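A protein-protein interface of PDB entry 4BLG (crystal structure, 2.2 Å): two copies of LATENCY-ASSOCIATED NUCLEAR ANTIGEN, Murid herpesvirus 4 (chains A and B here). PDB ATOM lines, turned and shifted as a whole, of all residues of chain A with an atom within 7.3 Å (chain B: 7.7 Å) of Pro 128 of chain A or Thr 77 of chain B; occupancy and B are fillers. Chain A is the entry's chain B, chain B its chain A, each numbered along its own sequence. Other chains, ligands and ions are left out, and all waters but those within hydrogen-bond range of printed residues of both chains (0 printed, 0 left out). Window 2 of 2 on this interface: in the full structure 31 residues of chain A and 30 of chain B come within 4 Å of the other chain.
Of the printed residues of chain B, Leu 127 of chain A touches Pro 72 (3.4 Å) and Val 74 (3.8 Å). Of chain B, only Val 74 (3.9 Å), Thr 77 (3.9 Å) and Gln 79 (3.0 Å) come within 4 Å of Pro 128 of chain A. Glu 129 of chain A touches none of the printed residues of chain B. Printed residues of chain A within 4 Å of Val 74 of chain B: Leu 127 and Pro 128. Of the printed residues of chain A, Pro 75 of chain B touches Pro 33. No residue of chain A comes within 4 Å of Gly 76 of chain B. Of the printed residues of chain A, Thr 77 of chain B touches Pro 128. Printed residues of chain A within 4 Å of Gln 79 of chain B: Pro 128. The nearest printed residue of chain A that does not touch Val 74 of chain B is Pro 33 of chain A (4.1 Å).
Hydrophobic or aromatic side chains of chain A that line the printed part of chain B: Pro 33, Leu 127 and Pro 128. Along chain A the printed residues that touch a printed residue of chain B span positions 33 to 128. Hydrophobic or aromatic side chains of chain B within 4 Å of the printed part of chain A: Leu 71 and Val 74.
No position is printed for both chains.
OE1 of Gln 79 of chain B lies close to O of Cys 81 of chain B, 3.0 Å away. The backbone NH of Leu 71 of chain B lies within hydrogen-bond range of the backbone carbonyl oxygen of Thr 83 of chain B (2.8 Å).
Among the printed residues, pairs that only touch across the chains: Pro 128 of chain A with Gln 79 of chain B, Leu 127 of chain A with Pro 72 of chain B, Pro 33 of chain A with Pro 75 of chain B, Pro 126 of chain A with Leu 71 of chain B, Leu 127 of chain A with Val 74 of chain B, Pro 128 of chain A with Val 74 of chain B and Pro 128 of chain A with Thr 77 of chain B.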
ATOM      1  N   PRO A  33      11.060  27.748 -22.887  1.00  0.00           N
ATOM      2  CA  PRO A  33       9.881  27.396 -22.093  1.00  0.00           C
ATOM      3  C   PRO A  33      10.270  26.455 -20.973  1.00  0.00           C
ATOM      4  O   PRO A  33      11.280  25.764 -21.088  1.00  0.00           O
ATOM      5  CB  PRO A  33       8.967  26.669 -23.092  1.00  0.00           C
ATOM      6  CG  PRO A  33       9.561  26.889 -24.441  1.00  0.00           C
ATOM      7  CD  PRO A  33      11.017  27.149 -24.232  1.00  0.00           C
ATOM      8  N   PRO A  34       9.484  26.431 -19.895  1.00  0.00           N
ATOM      9  CA  PRO A  34       9.703  25.398 -18.887  1.00  0.00           C
ATOM     10  C   PRO A  34       9.431  24.030 -19.497  1.00  0.00           C
ATOM     11  O   PRO A  34       8.831  23.945 -20.567  1.00  0.00           O
ATOM     12  CB  PRO A  34       8.668  25.737 -17.815  1.00  0.00           C
ATOM     13  CG  PRO A  34       7.584  26.442 -18.563  1.00  0.00           C
ATOM     14  CD  PRO A  34       8.312  27.264 -19.583  1.00  0.00           C
ATOM     15  N   THR A  35       9.870  22.975 -18.824  1.00  0.00           N
ATOM     16  CA  THR A  35       9.742  21.626 -19.356  1.00  0.00           C
ATOM     17  C   THR A  35       8.306  21.120 -19.222  1.00  0.00           C
ATOM     18  O   THR A  35       7.816  20.379 -20.073  1.00  0.00           O
ATOM     19  CB  THR A  35      10.712  20.679 -18.637  1.00  0.00           C
ATOM     20  OG1 THR A  35      12.034  21.231 -18.693  1.00  0.00           O
ATOM     21  CG2 THR A  35      10.706  19.302 -19.282  1.00  0.00           C
ATOM     22  N   HIS A  36       7.635  21.528 -18.152  1.00  0.00           N
ATOM     23  CA  HIS A  36       6.229  21.216 -17.970  1.00  0.00           C
ATOM     24  C   HIS A  36       5.504  22.426 -17.436  1.00  0.00           C
ATOM     25  O   HIS A  36       6.081  23.259 -16.739  1.00  0.00           O
ATOM     26  CB  HIS A  36       6.038  20.064 -16.989  1.00  0.00           C
ATOM     27  CG  HIS A  36       6.737  18.808 -17.392  1.00  0.00           C
ATOM     28  ND1 HIS A  36       6.535  18.205 -18.614  1.00  0.00           N
ATOM     29  CD2 HIS A  36       7.636  18.038 -16.735  1.00  0.00           C
ATOM     30  CE1 HIS A  36       7.281  17.118 -18.694  1.00  0.00           C
ATOM     31  NE2 HIS A  36       7.958  16.993 -17.566  1.00  0.00           N
ATOM     32  N   PHE A  37       4.228  22.509 -17.777  1.00  0.00           N
ATOM     33  CA  PHE A  37       3.348  23.523 -17.248  1.00  0.00           C
ATOM     34  C   PHE A  37       2.394  22.880 -16.256  1.00  0.00           C
ATOM     35  O   PHE A  37       1.366  22.324 -16.640  1.00  0.00           O
ATOM     36  CB  PHE A  37       2.581  24.165 -18.394  1.00  0.00           C
ATOM     37  CG  PHE A  37       3.440  24.995 -19.296  1.00  0.00           C
ATOM     38  CD1 PHE A  37       4.123  24.413 -20.351  1.00  0.00           C
ATOM     39  CD2 PHE A  37       3.569  26.354 -19.086  1.00  0.00           C
ATOM     40  CE1 PHE A  37       4.910  25.174 -21.183  1.00  0.00           C
ATOM     41  CE2 PHE A  37       4.356  27.127 -19.919  1.00  0.00           C
ATOM     42  CZ  PHE A  37       5.031  26.532 -20.969  1.00  0.00           C
ATOM     43  N   PHE A 125      -0.214  20.050 -17.365  1.00  0.00           N
ATOM     44  CA  PHE A 125      -1.097  20.276 -18.477  1.00  0.00           C
ATOM     45  C   PHE A 125      -0.587  19.616 -19.725  1.00  0.00           C
ATOM     46  O   PHE A 125       0.597  19.480 -19.910  1.00  0.00           O
ATOM     47  CB  PHE A 125      -1.336  21.748 -18.687  1.00  0.00           C
ATOM     48  CG  PHE A 125      -2.224  22.350 -17.667  1.00  0.00           C
ATOM     49  CD1 PHE A 125      -3.581  22.226 -17.770  1.00  0.00           C
ATOM     50  CD2 PHE A 125      -1.702  23.035 -16.610  1.00  0.00           C
ATOM     51  CE1 PHE A 125      -4.405  22.773 -16.834  1.00  0.00           C
ATOM     52  CE2 PHE A 125      -2.512  23.579 -15.670  1.00  0.00           C
ATOM     53  CZ  PHE A 125      -3.871  23.447 -15.783  1.00  0.00           C
ATOM     54  N   PRO A 126      -1.486  19.185 -20.584  1.00  0.00           N
ATOM     55  CA  PRO A 126      -1.117  18.426 -21.769  1.00  0.00           C
ATOM     56  C   PRO A 126      -0.566  19.246 -22.925  1.00  0.00           C
ATOM     57  O   PRO A 126      -1.069  19.196 -24.006  1.00  0.00           O
ATOM     58  CB  PRO A 126      -2.427  17.760 -22.164  1.00  0.00           C
ATOM     59  CG  PRO A 126      -3.462  18.642 -21.611  1.00  0.00           C
ATOM     60  CD  PRO A 126      -2.920  19.117 -20.320  1.00  0.00           C
ATOM     61  N   LEU A 127       0.514  19.955 -22.695  1.00  0.00           N
ATOM     62  CA  LEU A 127       1.212  20.645 -23.755  1.00  0.00           C
ATOM     63  C   LEU A 127       2.463  19.862 -24.128  1.00  0.00           C
ATOM     64  O   LEU A 127       3.117  19.326 -23.272  1.00  0.00           O
ATOM     65  CB  LEU A 127       1.574  22.033 -23.269  1.00  0.00           C
ATOM     66  CG  LEU A 127       0.406  22.905 -22.833  1.00  0.00           C
ATOM     67  CD1 LEU A 127       0.742  23.826 -21.702  1.00  0.00           C
ATOM     68  CD2 LEU A 127      -0.066  23.729 -23.991  1.00  0.00           C
ATOM     69  N   PRO A 128       2.791  19.806 -25.489  1.00  0.00           N
ATOM     70  CA  PRO A 128       4.007  19.016 -25.797  1.00  0.00           C
ATOM     71  C   PRO A 128       5.239  19.375 -25.016  1.00  0.00           C
ATOM     72  O   PRO A 128       5.264  20.410 -24.380  1.00  0.00           O
ATOM     73  CB  PRO A 128       4.303  19.368 -27.238  1.00  0.00           C
ATOM     74  CG  PRO A 128       3.626  20.645 -27.470  1.00  0.00           C
ATOM     75  CD  PRO A 128       2.325  20.344 -26.849  1.00  0.00           C
ATOM     76  N   GLU A 129       6.264  18.538 -25.070  1.00  0.00           N
ATOM     77  CA  GLU A 129       7.529  18.860 -24.423  1.00  0.00           C
ATOM     78  C   GLU A 129       8.612  19.179 -25.441  1.00  0.00           C
ATOM     79  O   GLU A 129       9.189  20.266 -25.431  1.00  0.00           O
ATOM     80  CB  GLU A 129       8.013  17.739 -23.509  1.00  0.00           C
ATOM     81  CG  GLU A 129       9.355  18.053 -22.861  1.00  0.00           C
ATOM     82  CD  GLU A 129      10.409  16.973 -23.056  1.00  0.00           C
ATOM     83  OE1 GLU A 129      11.082  16.946 -24.110  1.00  0.00           O
ATOM     84  OE2 GLU A 129      10.577  16.159 -22.132  1.00  0.00           O
ATOM     85  N   LEU B  71      -5.431  24.612 -27.294  1.00  0.00           N
ATOM     86  CA  LEU B  71      -4.296  24.912 -26.437  1.00  0.00           C
ATOM     87  C   LEU B  71      -3.281  25.753 -27.214  1.00  0.00           C
ATOM     88  O   LEU B  71      -3.168  25.640 -28.431  1.00  0.00           O
ATOM     89  CB  LEU B  71      -3.639  23.636 -25.929  1.00  0.00           C
ATOM     90  CG  LEU B  71      -4.512  22.774 -25.018  1.00  0.00           C
ATOM     91  CD1 LEU B  71      -3.807  21.462 -24.693  1.00  0.00           C
ATOM     92  CD2 LEU B  71      -4.868  23.522 -23.748  1.00  0.00           C
ATOM     93  N   PRO B  72      -2.540  26.612 -26.514  1.00  0.00           N
ATOM     94  CA  PRO B  72      -1.520  27.368 -27.243  1.00  0.00           C
ATOM     95  C   PRO B  72      -0.337  26.484 -27.615  1.00  0.00           C
ATOM     96  O   PRO B  72      -0.005  25.554 -26.883  1.00  0.00           O
ATOM     97  CB  PRO B  72      -1.089  28.433 -26.239  1.00  0.00           C
ATOM     98  CG  PRO B  72      -1.356  27.835 -24.910  1.00  0.00           C
ATOM     99  CD  PRO B  72      -2.542  26.917 -25.074  1.00  0.00           C
ATOM    100  N   LEU B  73       0.283  26.777 -28.750  1.00  0.00           N
ATOM    101  CA  LEU B  73       1.497  26.095 -29.162  1.00  0.00           C
ATOM    102  C   LEU B  73       2.653  26.433 -28.239  1.00  0.00           C
ATOM    103  O   LEU B  73       2.767  27.562 -27.757  1.00  0.00           O
ATOM    104  CB  LEU B  73       1.859  26.503 -30.588  1.00  0.00           C
ATOM    105  CG  LEU B  73       0.896  25.960 -31.638  1.00  0.00           C
ATOM    106  CD1 LEU B  73       1.260  26.507 -33.006  1.00  0.00           C
ATOM    107  CD2 LEU B  73       0.914  24.438 -31.629  1.00  0.00           C
ATOM    108  N   VAL B  74       3.518  25.450 -28.012  1.00  0.00           N
ATOM    109  CA  VAL B  74       4.711  25.652 -27.206  1.00  0.00           C
ATOM    110  C   VAL B  74       5.883  25.994 -28.112  1.00  0.00           C
ATOM    111  O   VAL B  74       6.269  25.191 -28.962  1.00  0.00           O
ATOM    112  CB  VAL B  74       5.061  24.400 -26.402  1.00  0.00           C
ATOM    113  CG1 VAL B  74       6.285  24.651 -25.536  1.00  0.00           C
ATOM    114  CG2 VAL B  74       3.876  23.974 -25.547  1.00  0.00           C
ATOM    115  N   PRO B  75       6.457  27.195 -27.932  1.00  0.00           N
ATOM    116  CA  PRO B  75       7.582  27.649 -28.754  1.00  0.00           C
ATOM    117  C   PRO B  75       8.719  26.637 -28.801  1.00  0.00           C
ATOM    118  O   PRO B  75       9.114  26.113 -27.760  1.00  0.00           O
ATOM    119  CB  PRO B  75       8.042  28.920 -28.035  1.00  0.00           C
ATOM    120  CG  PRO B  75       6.824  29.422 -27.352  1.00  0.00           C
ATOM    121  CD  PRO B  75       6.059  28.204 -26.936  1.00  0.00           C
ATOM    122  N   GLY B  76       9.232  26.367 -29.997  1.00  0.00           N
ATOM    123  CA  GLY B  76      10.397  25.513 -30.152  1.00  0.00           C
ATOM    124  C   GLY B  76      10.117  24.049 -29.870  1.00  0.00           C
ATOM    125  O   GLY B  76      10.779  23.428 -29.037  1.00  0.00           O
ATOM    126  N   THR B  77       9.133  23.495 -30.571  1.00  0.00           N
ATOM    127  CA  THR B  77       8.807  22.082 -30.436  1.00  0.00           C
ATOM    128  C   THR B  77       8.429  21.526 -31.802  1.00  0.00           C
ATOM    129  O   THR B  77       8.406  22.253 -32.795  1.00  0.00           O
ATOM    130  CB  THR B  77       7.658  21.851 -29.436  1.00  0.00           C
ATOM    131  OG1 THR B  77       7.578  20.459 -29.099  1.00  0.00           O
ATOM    132  CG2 THR B  77       6.336  22.310 -30.027  1.00  0.00           C
ATOM    133  N   THR B  78       8.123  20.234 -31.841  1.00  0.00           N
ATOM    134  CA  THR B  78       7.954  19.533 -33.103  1.00  0.00           C
ATOM    135  C   THR B  78       6.557  18.926 -33.225  1.00  0.00           C
ATOM    136  O   THR B  78       6.409  17.706 -33.267  1.00  0.00           O
ATOM    137  CB  THR B  78       9.020  18.420 -33.240  1.00  0.00           C
ATOM    138  OG1 THR B  78       8.620  17.263 -32.494  1.00  0.00           O
ATOM    139  CG2 THR B  78      10.369  18.905 -32.717  1.00  0.00           C
ATOM    140  N   GLN B  79       5.533  19.777 -33.283  1.00  0.00           N
ATOM    141  CA  GLN B  79       4.161  19.296 -33.430  1.00  0.00           C
ATOM    142  C   GLN B  79       3.476  19.842 -34.681  1.00  0.00           C
ATOM    143  O   GLN B  79       2.936  19.074 -35.481  1.00  0.00           O
ATOM    144  CB  GLN B  79       3.328  19.620 -32.182  1.00  0.00           C
ATOM    145  CG  GLN B  79       3.218  21.100 -31.837  1.00  0.00           C
ATOM    146  CD  GLN B  79       2.336  21.351 -30.623  1.00  0.00           C
ATOM    147  OE1 GLN B  79       1.336  20.661 -30.412  1.00  0.00           O
ATOM    148  NE2 GLN B  79       2.706  22.342 -29.817  1.00  0.00           N
ATOM    149  N   GLN B  80       3.499  21.161 -34.849  1.00  0.00           N
ATOM    150  CA  GLN B  80       2.783  21.806 -35.946  1.00  0.00           C
ATOM    151  C   GLN B  80       1.359  21.260 -36.065  1.00  0.00           C
ATOM    152  O   GLN B  80       0.756  21.297 -37.135  1.00  0.00           O
ATOM    153  CB  GLN B  80       3.526  21.604 -37.267  1.00  0.00           C
ATOM    154  CG  GLN B  80       3.706  22.878 -38.082  1.00  0.00           C
ATOM    155  CD  GLN B  80       4.556  22.659 -39.321  1.00  0.00           C
ATOM    156  OE1 GLN B  80       5.028  21.551 -39.569  1.00  0.00           O
ATOM    157  NE2 GLN B  80       4.757  23.714 -40.106  1.00  0.00           N
ATOM    158  N   CYS B  81       0.833  20.798 -34.956  1.00  0.00           N
ATOM    159  CA  CYS B  81      -0.510  20.302 -34.922  1.00  0.00           C
ATOM    160  C   CYS B  81      -1.161  20.901 -33.717  1.00  0.00           C
ATOM    161  O   CYS B  81      -0.688  20.716 -32.619  1.00  0.00           O
ATOM    162  CB  CYS B  81      -0.455  18.808 -34.738  1.00  0.00           C
ATOM    163  SG  CYS B  81      -1.882  18.007 -35.407  1.00  0.00           S
ATOM    164  N   THR B  83      -3.523  21.272 -30.623  1.00  0.00           N
ATOM    165  CA  THR B  83      -4.162  20.348 -29.712  1.00  0.00           C
ATOM    166  C   THR B  83      -5.390  21.050 -29.154  1.00  0.00           C
ATOM    167  O   THR B  83      -5.291  22.145 -28.600  1.00  0.00           O
ATOM    168  CB  THR B  83      -3.206  19.940 -28.597  1.00  0.00           C
ATOM    169  OG1 THR B  83      -2.100  19.243 -29.175  1.00  0.00           O
ATOM    170  CG2 THR B  83      -3.902  19.046 -27.578  1.00  0.00           C
